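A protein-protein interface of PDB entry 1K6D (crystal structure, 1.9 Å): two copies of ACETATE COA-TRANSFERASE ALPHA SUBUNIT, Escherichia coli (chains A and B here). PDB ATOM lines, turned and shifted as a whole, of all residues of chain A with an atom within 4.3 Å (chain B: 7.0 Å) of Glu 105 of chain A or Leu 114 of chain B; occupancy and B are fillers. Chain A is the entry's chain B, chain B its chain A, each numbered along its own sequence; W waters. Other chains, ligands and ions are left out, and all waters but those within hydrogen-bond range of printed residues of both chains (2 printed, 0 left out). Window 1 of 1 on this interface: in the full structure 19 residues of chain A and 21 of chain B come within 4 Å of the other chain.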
ATOM      1  N   GLY A 101       0.033 -37.593 -19.379  1.00  0.00           N
ATOM      2  CA  GLY A 101      -0.527 -36.579 -18.498  1.00  0.00           C
ATOM      3  C   GLY A 101      -1.496 -35.692 -19.247  1.00  0.00           C
ATOM      4  O   GLY A 101      -2.494 -35.227 -18.708  1.00  0.00           O
ATOM      5  N   THR A 102      -1.171 -35.423 -20.507  1.00  0.00           N
ATOM      6  CA  THR A 102      -2.028 -34.592 -21.336  1.00  0.00           C
ATOM      7  C   THR A 102      -3.339 -35.307 -21.643  1.00  0.00           C
ATOM      8  O   THR A 102      -4.414 -34.725 -21.504  1.00  0.00           O
ATOM      9  CB  THR A 102      -1.285 -34.202 -22.646  1.00  0.00           C
ATOM     10  OG1 THR A 102      -0.189 -33.340 -22.305  1.00  0.00           O
ATOM     11  CG2 THR A 102      -2.220 -33.482 -23.618  1.00  0.00           C
ATOM     12  N   LEU A 103      -3.253 -36.580 -22.030  1.00  0.00           N
ATOM     13  CA  LEU A 103      -4.462 -37.363 -22.364  1.00  0.00           C
ATOM     14  C   LEU A 103      -5.409 -37.411 -21.156  1.00  0.00           C
ATOM     15  O   LEU A 103      -6.618 -37.243 -21.281  1.00  0.00           O
ATOM     16  CB  LEU A 103      -4.059 -38.781 -22.794  1.00  0.00           C
ATOM     17  CG  LEU A 103      -5.193 -39.753 -23.179  1.00  0.00           C
ATOM     18  CD1 LEU A 103      -6.080 -39.154 -24.269  1.00  0.00           C
ATOM     19  CD2 LEU A 103      -4.568 -41.061 -23.647  1.00  0.00           C
ATOM     20  N   ILE A 104      -4.839 -37.604 -19.973  1.00  0.00           N
ATOM     21  CA  ILE A 104      -5.634 -37.644 -18.753  1.00  0.00           C
ATOM     22  C   ILE A 104      -6.369 -36.324 -18.546  1.00  0.00           C
ATOM     23  O   ILE A 104      -7.576 -36.303 -18.295  1.00  0.00           O
ATOM     24  CB  ILE A 104      -4.728 -37.952 -17.527  1.00  0.00           C
ATOM     25  CG1 ILE A 104      -4.246 -39.402 -17.624  1.00  0.00           C
ATOM     26  CG2 ILE A 104      -5.470 -37.636 -16.209  1.00  0.00           C
ATOM     27  CD1 ILE A 104      -3.078 -39.759 -16.698  1.00  0.00           C
ATOM     28  N   GLU A 105      -5.652 -35.209 -18.670  1.00  0.00           N
ATOM     29  CA  GLU A 105      -6.278 -33.911 -18.460  1.00  0.00           C
ATOM     30  C   GLU A 105      -7.301 -33.568 -19.549  1.00  0.00           C
ATOM     31  O   GLU A 105      -8.278 -32.866 -19.290  1.00  0.00           O
ATOM     32  CB  GLU A 105      -5.208 -32.823 -18.357  1.00  0.00           C
ATOM     33  CG  GLU A 105      -5.778 -31.429 -18.090  1.00  0.00           C
ATOM     34  CD  GLU A 105      -6.430 -31.269 -16.711  1.00  0.00           C
ATOM     35  OE1 GLU A 105      -6.405 -32.225 -15.896  1.00  0.00           O
ATOM     36  OE2 GLU A 105      -6.965 -30.170 -16.441  1.00  0.00           O
ATOM     37  N   GLN A 106      -7.076 -34.036 -20.776  1.00  0.00           N
ATOM     38  CA  GLN A 106      -8.042 -33.774 -21.836  1.00  0.00           C
ATOM     39  C   GLN A 106      -9.370 -34.454 -21.475  1.00  0.00           C
ATOM     40  O   GLN A 106     -10.454 -33.868 -21.587  1.00  0.00           O
ATOM     41  CB  GLN A 106      -7.541 -34.343 -23.172  1.00  0.00           C
ATOM     42  CG  GLN A 106      -6.455 -33.497 -23.822  1.00  0.00           C
ATOM     43  CD  GLN A 106      -6.084 -34.009 -25.187  1.00  0.00           C
ATOM     44  OE1 GLN A 106      -5.261 -34.920 -25.326  1.00  0.00           O
ATOM     45  NE2 GLN A 106      -6.711 -33.437 -26.217  1.00  0.00           N
ATOM     46  N   ILE A 107      -9.271 -35.707 -21.067  1.00  0.00           N
ATOM     47  CA  ILE A 107     -10.477 -36.448 -20.696  1.00  0.00           C
ATOM     48  C   ILE A 107     -11.108 -35.825 -19.456  1.00  0.00           C
ATOM     49  O   ILE A 107     -12.334 -35.714 -19.359  1.00  0.00           O
ATOM     50  CB  ILE A 107     -10.161 -37.929 -20.461  1.00  0.00           C
ATOM     51  CG1 ILE A 107      -9.573 -38.528 -21.744  1.00  0.00           C
ATOM     52  CG2 ILE A 107     -11.452 -38.670 -19.993  1.00  0.00           C
ATOM     53  CD1 ILE A 107      -9.150 -39.978 -21.642  1.00  0.00           C
ATOM     54  N   ARG A 108     -10.288 -35.368 -18.516  1.00  0.00           N
ATOM     55  CA  ARG A 108     -10.860 -34.755 -17.316  1.00  0.00           C
ATOM     56  C   ARG A 108     -11.606 -33.485 -17.701  1.00  0.00           C
ATOM     57  O   ARG A 108     -12.692 -33.221 -17.180  1.00  0.00           O
ATOM     58  CB  ARG A 108      -9.774 -34.437 -16.289  1.00  0.00           C
ATOM     59  CG  ARG A 108     -10.345 -34.083 -14.895  1.00  0.00           C
ATOM     60  CD  ARG A 108      -9.256 -33.521 -13.994  1.00  0.00           C
ATOM     61  NE  ARG A 108      -8.897 -32.186 -14.450  1.00  0.00           N
ATOM     62  CZ  ARG A 108      -9.673 -31.118 -14.278  1.00  0.00           C
ATOM     63  NH1 ARG A 108     -10.831 -31.234 -13.642  1.00  0.00           N
ATOM     64  NH2 ARG A 108      -9.325 -29.946 -14.791  1.00  0.00           N
ATOM     65  N   CYS A 109     -11.038 -32.688 -18.611  1.00  0.00           N
ATOM     66  CA  CYS A 109     -11.727 -31.472 -19.046  1.00  0.00           C
ATOM     67  C   CYS A 109     -13.040 -31.831 -19.740  1.00  0.00           C
ATOM     68  O   CYS A 109     -14.050 -31.142 -19.565  1.00  0.00           O
ATOM     69  CB  CYS A 109     -10.846 -30.645 -20.003  1.00  0.00           C
ATOM     70  SG  CYS A 109      -9.593 -29.679 -19.149  1.00  0.00           S
ATOM     71  N   PHE A 117      -7.039 -26.496 -21.827  1.00  0.00           N
ATOM     72  CA  PHE A 117      -6.080 -26.100 -20.807  1.00  0.00           C
ATOM     73  C   PHE A 117      -4.706 -25.826 -21.391  1.00  0.00           C
ATOM     74  O   PHE A 117      -4.410 -26.214 -22.528  1.00  0.00           O
ATOM     75  CB  PHE A 117      -5.968 -27.187 -19.732  1.00  0.00           C
ATOM     76  CG  PHE A 117      -5.504 -28.525 -20.258  1.00  0.00           C
ATOM     77  CD1 PHE A 117      -6.393 -29.393 -20.906  1.00  0.00           C
ATOM     78  CD2 PHE A 117      -4.176 -28.909 -20.123  1.00  0.00           C
ATOM     79  CE1 PHE A 117      -5.946 -30.626 -21.412  1.00  0.00           C
ATOM     80  CE2 PHE A 117      -3.720 -30.134 -20.625  1.00  0.00           C
ATOM     81  CZ  PHE A 117      -4.607 -30.992 -21.268  1.00  0.00           C
ATOM     82  N   LEU A 118      -3.877 -25.134 -20.611  1.00  0.00           N
ATOM     83  CA  LEU A 118      -2.521 -24.806 -21.029  1.00  0.00           C
ATOM     84  C   LEU A 118      -1.582 -25.740 -20.290  1.00  0.00           C
ATOM     85  O   LEU A 118      -1.665 -25.891 -19.069  1.00  0.00           O
ATOM     86  CB  LEU A 118      -2.187 -23.350 -20.684  1.00  0.00           C
ATOM     87  CG  LEU A 118      -3.058 -22.269 -21.335  1.00  0.00           C
ATOM     88  CD1 LEU A 118      -2.616 -20.886 -20.853  1.00  0.00           C
ATOM     89  CD2 LEU A 118      -2.949 -22.381 -22.838  1.00  0.00           C
ATOM     90  N   THR A 119      -0.681 -26.369 -21.028  1.00  0.00           N
ATOM     91  CA  THR A 119       0.260 -27.300 -20.421  1.00  0.00           C
ATOM     92  C   THR A 119       1.685 -27.094 -20.907  1.00  0.00           C
ATOM     93  O   THR A 119       1.910 -26.651 -22.025  1.00  0.00           O
ATOM     94  CB  THR A 119      -0.110 -28.768 -20.738  1.00  0.00           C
ATOM     95  OG1 THR A 119       0.877 -29.630 -20.165  1.00  0.00           O
ATOM     96  CG2 THR A 119      -0.155 -29.011 -22.240  1.00  0.00           C
ATOM     97  N   TRP A 141       3.122 -22.062 -23.215  1.00  0.00           N
ATOM     98  CA  TRP A 141       2.297 -23.227 -22.923  1.00  0.00           C
ATOM     99  C   TRP A 141       1.548 -23.708 -24.149  1.00  0.00           C
ATOM    100  O   TRP A 141       1.166 -22.912 -25.007  1.00  0.00           O
ATOM    101  CB  TRP A 141       1.247 -22.884 -21.857  1.00  0.00           C
ATOM    102  CG  TRP A 141       1.743 -22.124 -20.666  1.00  0.00           C
ATOM    103  CD1 TRP A 141       1.904 -20.775 -20.567  1.00  0.00           C
ATOM    104  CD2 TRP A 141       2.082 -22.666 -19.388  1.00  0.00           C
ATOM    105  NE1 TRP A 141       2.312 -20.438 -19.301  1.00  0.00           N
ATOM    106  CE2 TRP A 141       2.431 -21.580 -18.554  1.00  0.00           C
ATOM    107  CE3 TRP A 141       2.121 -23.964 -18.861  1.00  0.00           C
ATOM    108  CZ2 TRP A 141       2.816 -21.751 -17.220  1.00  0.00           C
ATOM    109  CZ3 TRP A 141       2.504 -24.135 -17.536  1.00  0.00           C
ATOM    110  CH2 TRP A 141       2.845 -23.030 -16.730  1.00  0.00           C
ATOM    111  N   GLU B 105     -10.950 -25.724  -9.557  1.00  0.00           N
ATOM    112  CA  GLU B 105     -10.158 -25.987 -10.769  1.00  0.00           C
ATOM    113  C   GLU B 105      -8.803 -25.263 -10.772  1.00  0.00           C
ATOM    114  O   GLU B 105      -7.814 -25.791 -11.279  1.00  0.00           O
ATOM    115  CB  GLU B 105     -10.947 -25.593 -12.022  1.00  0.00           C
ATOM    116  CG  GLU B 105     -12.113 -26.506 -12.366  1.00  0.00           C
ATOM    117  CD  GLU B 105     -11.691 -27.945 -12.591  1.00  0.00           C
ATOM    118  OE1 GLU B 105     -10.488 -28.193 -12.843  1.00  0.00           O
ATOM    119  OE2 GLU B 105     -12.570 -28.830 -12.529  1.00  0.00           O
ATOM    120  N   ARG B 108      -6.599 -27.271  -8.546  1.00  0.00           N
ATOM    121  CA  ARG B 108      -6.299 -28.541  -9.215  1.00  0.00           C
ATOM    122  C   ARG B 108      -5.264 -28.293 -10.315  1.00  0.00           C
ATOM    123  O   ARG B 108      -4.326 -29.057 -10.485  1.00  0.00           O
ATOM    124  CB  ARG B 108      -7.556 -29.124  -9.844  1.00  0.00           C
ATOM    125  CG  ARG B 108      -7.364 -30.542 -10.367  1.00  0.00           C
ATOM    126  CD  ARG B 108      -8.525 -30.942 -11.245  1.00  0.00           C
ATOM    127  NE  ARG B 108      -9.792 -30.653 -10.596  1.00  0.00           N
ATOM    128  CZ  ARG B 108     -10.251 -31.303  -9.535  1.00  0.00           C
ATOM    129  NH1 ARG B 108      -9.543 -32.287  -8.995  1.00  0.00           N
ATOM    130  NH2 ARG B 108     -11.427 -30.976  -9.024  1.00  0.00           N
ATOM    131  N   CYS B 109      -5.450 -27.200 -11.048  1.00  0.00           N
ATOM    132  CA  CYS B 109      -4.547 -26.818 -12.132  1.00  0.00           C
ATOM    133  C   CYS B 109      -3.134 -26.610 -11.563  1.00  0.00           C
ATOM    134  O   CYS B 109      -2.142 -27.088 -12.132  1.00  0.00           O
ATOM    135  CB  CYS B 109      -5.095 -25.527 -12.779  1.00  0.00           C
ATOM    136  SG  CYS B 109      -4.251 -24.950 -14.282  1.00  0.00           S
ATOM    137  N   GLY B 110      -3.043 -25.932 -10.416  1.00  0.00           N
ATOM    138  CA  GLY B 110      -1.740 -25.695  -9.807  1.00  0.00           C
ATOM    139  C   GLY B 110      -1.049 -26.985  -9.362  1.00  0.00           C
ATOM    140  O   GLY B 110       0.174 -27.117  -9.458  1.00  0.00           O
ATOM    141  N   GLY B 111      -1.833 -27.931  -8.860  1.00  0.00           N
ATOM    142  CA  GLY B 111      -1.272 -29.192  -8.407  1.00  0.00           C
ATOM    143  C   GLY B 111      -0.879 -30.091  -9.572  1.00  0.00           C
ATOM    144  O   GLY B 111      -0.051 -30.988  -9.415  1.00  0.00           O
ATOM    145  N   ALA B 112      -1.472 -29.850 -10.739  1.00  0.00           N
ATOM    146  CA  ALA B 112      -1.186 -30.643 -11.928  1.00  0.00           C
ATOM    147  C   ALA B 112      -0.021 -30.053 -12.715  1.00  0.00           C
ATOM    148  O   ALA B 112       0.413 -30.616 -13.715  1.00  0.00           O
ATOM    149  CB  ALA B 112      -2.432 -30.718 -12.818  1.00  0.00           C
ATOM    150  N   GLY B 113       0.476 -28.909 -12.268  1.00  0.00           N
ATOM    151  CA  GLY B 113       1.594 -28.274 -12.946  1.00  0.00           C
ATOM    152  C   GLY B 113       1.222 -27.669 -14.289  1.00  0.00           C
ATOM    153  O   GLY B 113       2.081 -27.515 -15.156  1.00  0.00           O
ATOM    154  N   LEU B 114      -0.050 -27.322 -14.463  1.00  0.00           N
ATOM    155  CA  LEU B 114      -0.526 -26.738 -15.714  1.00  0.00           C
ATOM    156  C   LEU B 114      -0.471 -25.211 -15.671  1.00  0.00           C
ATOM    157  O   LEU B 114      -0.278 -24.629 -14.593  1.00  0.00           O
ATOM    158  CB  LEU B 114      -1.948 -27.211 -15.994  1.00  0.00           C
ATOM    159  CG  LEU B 114      -2.078 -28.731 -16.125  1.00  0.00           C
ATOM    160  CD1 LEU B 114      -3.561 -29.103 -16.219  1.00  0.00           C
ATOM    161  CD2 LEU B 114      -1.279 -29.228 -17.332  1.00  0.00           C
ATOM    162  N   GLY B 115      -0.650 -24.570 -16.834  1.00  0.00           N
ATOM    163  CA  GLY B 115      -0.579 -23.119 -16.901  1.00  0.00           C
ATOM    164  C   GLY B 115      -1.883 -22.346 -16.883  1.00  0.00           C
ATOM    165  O   GLY B 115      -1.862 -21.111 -16.896  1.00  0.00           O
ATOM    166  N   GLY B 116      -3.010 -23.054 -16.856  1.00  0.00           N
ATOM    167  CA  GLY B 116      -4.305 -22.407 -16.827  1.00  0.00           C
ATOM    168  C   GLY B 116      -5.354 -23.270 -17.504  1.00  0.00           C
ATOM    169  O   GLY B 116      -5.026 -24.309 -18.092  1.00  0.00           O
ATOM    170  N   PHE B 117      -6.613 -22.852 -17.422  1.00  0.00           N
ATOM    171  CA  PHE B 117      -7.690 -23.601 -18.043  1.00  0.00           C
ATOM    172  C   PHE B 117      -8.753 -22.670 -18.555  1.00  0.00           C
ATOM    173  O   PHE B 117      -8.824 -21.503 -18.153  1.00  0.00           O
ATOM    174  CB  PHE B 117      -8.325 -24.601 -17.066  1.00  0.00           C
ATOM    175  CG  PHE B 117      -8.900 -23.969 -15.830  1.00  0.00           C
ATOM    176  CD1 PHE B 117      -8.081 -23.603 -14.772  1.00  0.00           C
ATOM    177  CD2 PHE B 117     -10.271 -23.755 -15.722  1.00  0.00           C
ATOM    178  CE1 PHE B 117      -8.619 -23.033 -13.611  1.00  0.00           C
ATOM    179  CE2 PHE B 117     -10.819 -23.186 -14.571  1.00  0.00           C
ATOM    180  CZ  PHE B 117      -9.985 -22.826 -13.513  1.00  0.00           C
ATOM    181  N   ARG B 145      -6.073 -18.872 -14.237  1.00  0.00           N
ATOM    182  CA  ARG B 145      -4.715 -19.306 -13.962  1.00  0.00           C
ATOM    183  C   ARG B 145      -4.609 -20.247 -12.763  1.00  0.00           C
ATOM    184  O   ARG B 145      -5.494 -20.300 -11.915  1.00  0.00           O
ATOM    185  CB  ARG B 145      -3.814 -18.084 -13.756  1.00  0.00           C
ATOM    186  CG  ARG B 145      -3.777 -17.142 -14.967  1.00  0.00           C
ATOM    187  CD  ARG B 145      -3.599 -17.937 -16.277  1.00  0.00           C
ATOM    188  NE  ARG B 145      -2.222 -18.010 -16.774  1.00  0.00           N
ATOM    189  CZ  ARG B 145      -1.143 -18.284 -16.044  1.00  0.00           C
ATOM    190  NH1 ARG B 145      -1.240 -18.514 -14.743  1.00  0.00           N
ATOM    191  NH2 ARG B 145       0.046 -18.356 -16.625  1.00  0.00           N
ATOM    192  N   PRO B 146      -3.532 -21.029 -12.705  1.00  0.00           N
ATOM    193  CA  PRO B 146      -3.374 -21.946 -11.574  1.00  0.00           C
ATOM    194  C   PRO B 146      -3.062 -21.221 -10.280  1.00  0.00           C
ATOM    195  O   PRO B 146      -2.559 -20.088 -10.283  1.00  0.00           O
ATOM    196  CB  PRO B 146      -2.212 -22.826 -12.007  1.00  0.00           C
ATOM    197  CG  PRO B 146      -1.381 -21.883 -12.864  1.00  0.00           C
ATOM    198  CD  PRO B 146      -2.458 -21.229 -13.696  1.00  0.00           C
ATOM    199  N   LEU B 147      -3.369 -21.887  -9.173  1.00  0.00           N
ATOM    200  CA  LEU B 147      -3.077 -21.358  -7.844  1.00  0.00           C
ATOM    201  C   LEU B 147      -2.238 -22.415  -7.126  1.00  0.00           C
ATOM    202  O   LEU B 147      -2.600 -23.592  -7.133  1.00  0.00           O
ATOM    203  CB  LEU B 147      -4.367 -21.153  -7.032  1.00  0.00           C
ATOM    204  CG  LEU B 147      -5.209 -19.890  -7.199  1.00  0.00           C
ATOM    205  CD1 LEU B 147      -6.455 -19.987  -6.316  1.00  0.00           C
ATOM    206  CD2 LEU B 147      -4.374 -18.680  -6.812  1.00  0.00           C
ATOM    207  N   ARG B 148      -1.128 -21.987  -6.536  1.00  0.00           N
ATOM    208  CA  ARG B 148      -0.263 -22.865  -5.744  1.00  0.00           C
ATOM    209  C   ARG B 148       0.049 -22.126  -4.440  1.00  0.00           C
ATOM    210  O   ARG B 148      -0.286 -20.949  -4.292  1.00  0.00           O
ATOM    211  CB  ARG B 148       1.035 -23.198  -6.497  1.00  0.00           C
ATOM    212  CG  ARG B 148       0.853 -24.292  -7.565  1.00  0.00           C
ATOM    213  CD  ARG B 148       2.198 -24.771  -8.124  1.00  0.00           C
ATOM    214  NE  ARG B 148       3.039 -25.361  -7.085  1.00  0.00           N
ATOM    215  CZ  ARG B 148       2.920 -26.611  -6.644  1.00  0.00           C
ATOM    216  NH1 ARG B 148       2.000 -27.420  -7.158  1.00  0.00           N
ATOM    217  NH2 ARG B 148       3.701 -27.041  -5.665  1.00  0.00           N
HETATM  218  O   HOH W   1      -6.311 -27.256 -15.675  1.00  0.00           O
HETATM  219  O   HOH W   2      -8.032 -27.544 -13.324  1.00  0.00           O
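Glu 105 of chain A touches just one residue of chain B: Leu 114 (3.6 Å).
Of the printed residues of chain B, Phe 117 of chain A touches Leu 114 (3.96 Å) and Gly 116 (3.4 Å).
Printed residues of chain A within 4 Å of Glu 105 of chain B: Arg 108.
Leu 114 of chain B touches just these residues of chain A: Glu 105, Phe 117, Leu 118, Thr 119 and Trp 141.
The nearest printed residue of chain B that does not touch Glu 105 of chain A is Ala 112 of chain B (5.2 Å).
The nearest printed residue of chain A that does not touch Leu 114 of chain B is Arg 108 of chain A (6.0 Å).
The side-chain carboxylate of Glu 105 of chain B lies within salt-bridge range of the guanidinium group of Arg 108 of chain B (3.4 Å).
The backbone NH (N) of Leu 114 of chain B lies within hydrogen-bond range of the backbone carbonyl oxygen (O) of Cys 109 of chain B (3.1 Å).
N of Gly 116 of chain B lies within hydrogen-bond range of SG of Cys 109 of chain B (3.4 Å).
The backbone carbonyl oxygen (O) of Gly 115 of chain B sits close to the guanidinium group (NE) of Arg 145 of chain B (3.1 Å).
The side-chain carboxylate (OE1) of Glu 105 of chain A is in salt-bridge range of the guanidinium group (NE) of Arg 108 of chain A, 2.9 Å away.
The backbone carbonyl oxygen (O) of Glu 105 of chain A is in hydrogen-bond range of the side-chain sulfur (SG) of Cys 109 of chain A, 3.5 Å away.
OE2 of Glu 105 of chain A touches CD1 of Leu 114 of chain B, 3.6 Å away.
Phe 117 of chain A touches Leu 114 of chain B.
CA of Phe 117 of chain A touches O of Gly 116 of chain B, at 3.4 Å.
Leu 118 of chain A touches Leu 114 of chain B.
Thr 119 of chain A touches Leu 114 of chain B (OG1 to CD2, 3.6 Å).
Trp 141 of chain A touches Leu 114 of chain B.
Trp 141 of chain A touches Gly 115 of chain B (CZ3 to N, 3.3 Å).
Water W2 lies within hydrogen-bond range of the side-chain carboxylate (OE1) of Glu 105 of chain B (2.6 Å), the guanidinium group (NH2) of Arg 108 of chain A (3.1 Å) and the backbone NH (N) of Cys 109 of chain B (3.5 Å).
Water W1 lies within hydrogen-bond range of OE2 of Glu 105 of chain A (3.1 Å) and SG of Cys 109 of chain B (3.4 Å).
Arg 108 of chain A touches Glu 105 of chain B, but with the chains exchanged Glu 105 of chain A does not touch Arg 108 of chain B (5.3 Å).
Arg 108 of chain A touches its own counterpart, Arg 108 of chain B.
The side-chain carboxylate (OE1) of Glu 105 of chain B is in salt-bridge range of the guanidinium group (NH2) of Arg 108 of chain A (2.9 Å).
The backbone NH (N) of Gly 115 of chain B sits at hydrogen-bond distance from the backbone carbonyl oxygen (O) of Leu 118 of chain A (2.8 Å).
The backbone carbonyl oxygen (O) of Gly 116 of chain B sits at hydrogen-bond distance from the backbone NH (N) of Leu 118 of chain A (2.9 Å).
NE of Arg 108 of chain B sits close to NH1 of Arg 108 of chain A, at 3.3 Å.
Of the 13 printed residues of chain A, 6 touch a printed residue of chain B.
Printed residues of chain A that touch a printed residue of chain B: Glu 105, Arg 108, Phe 117, Leu 118, Thr 119 and Trp 141.
Hydrophobic or aromatic side chains of chain A that line the printed part of chain B: Phe 117, Leu 118 and Trp 141.
Along chain A the printed residues that touch a printed residue of chain B span positions 105 to 141.
Of the 15 printed residues of chain B, 5 touch a printed residue of chain A.
Printed residues of chain B that touch a printed residue of chain A: Glu 105, Arg 108, Leu 114, Gly 115 and Gly 116.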
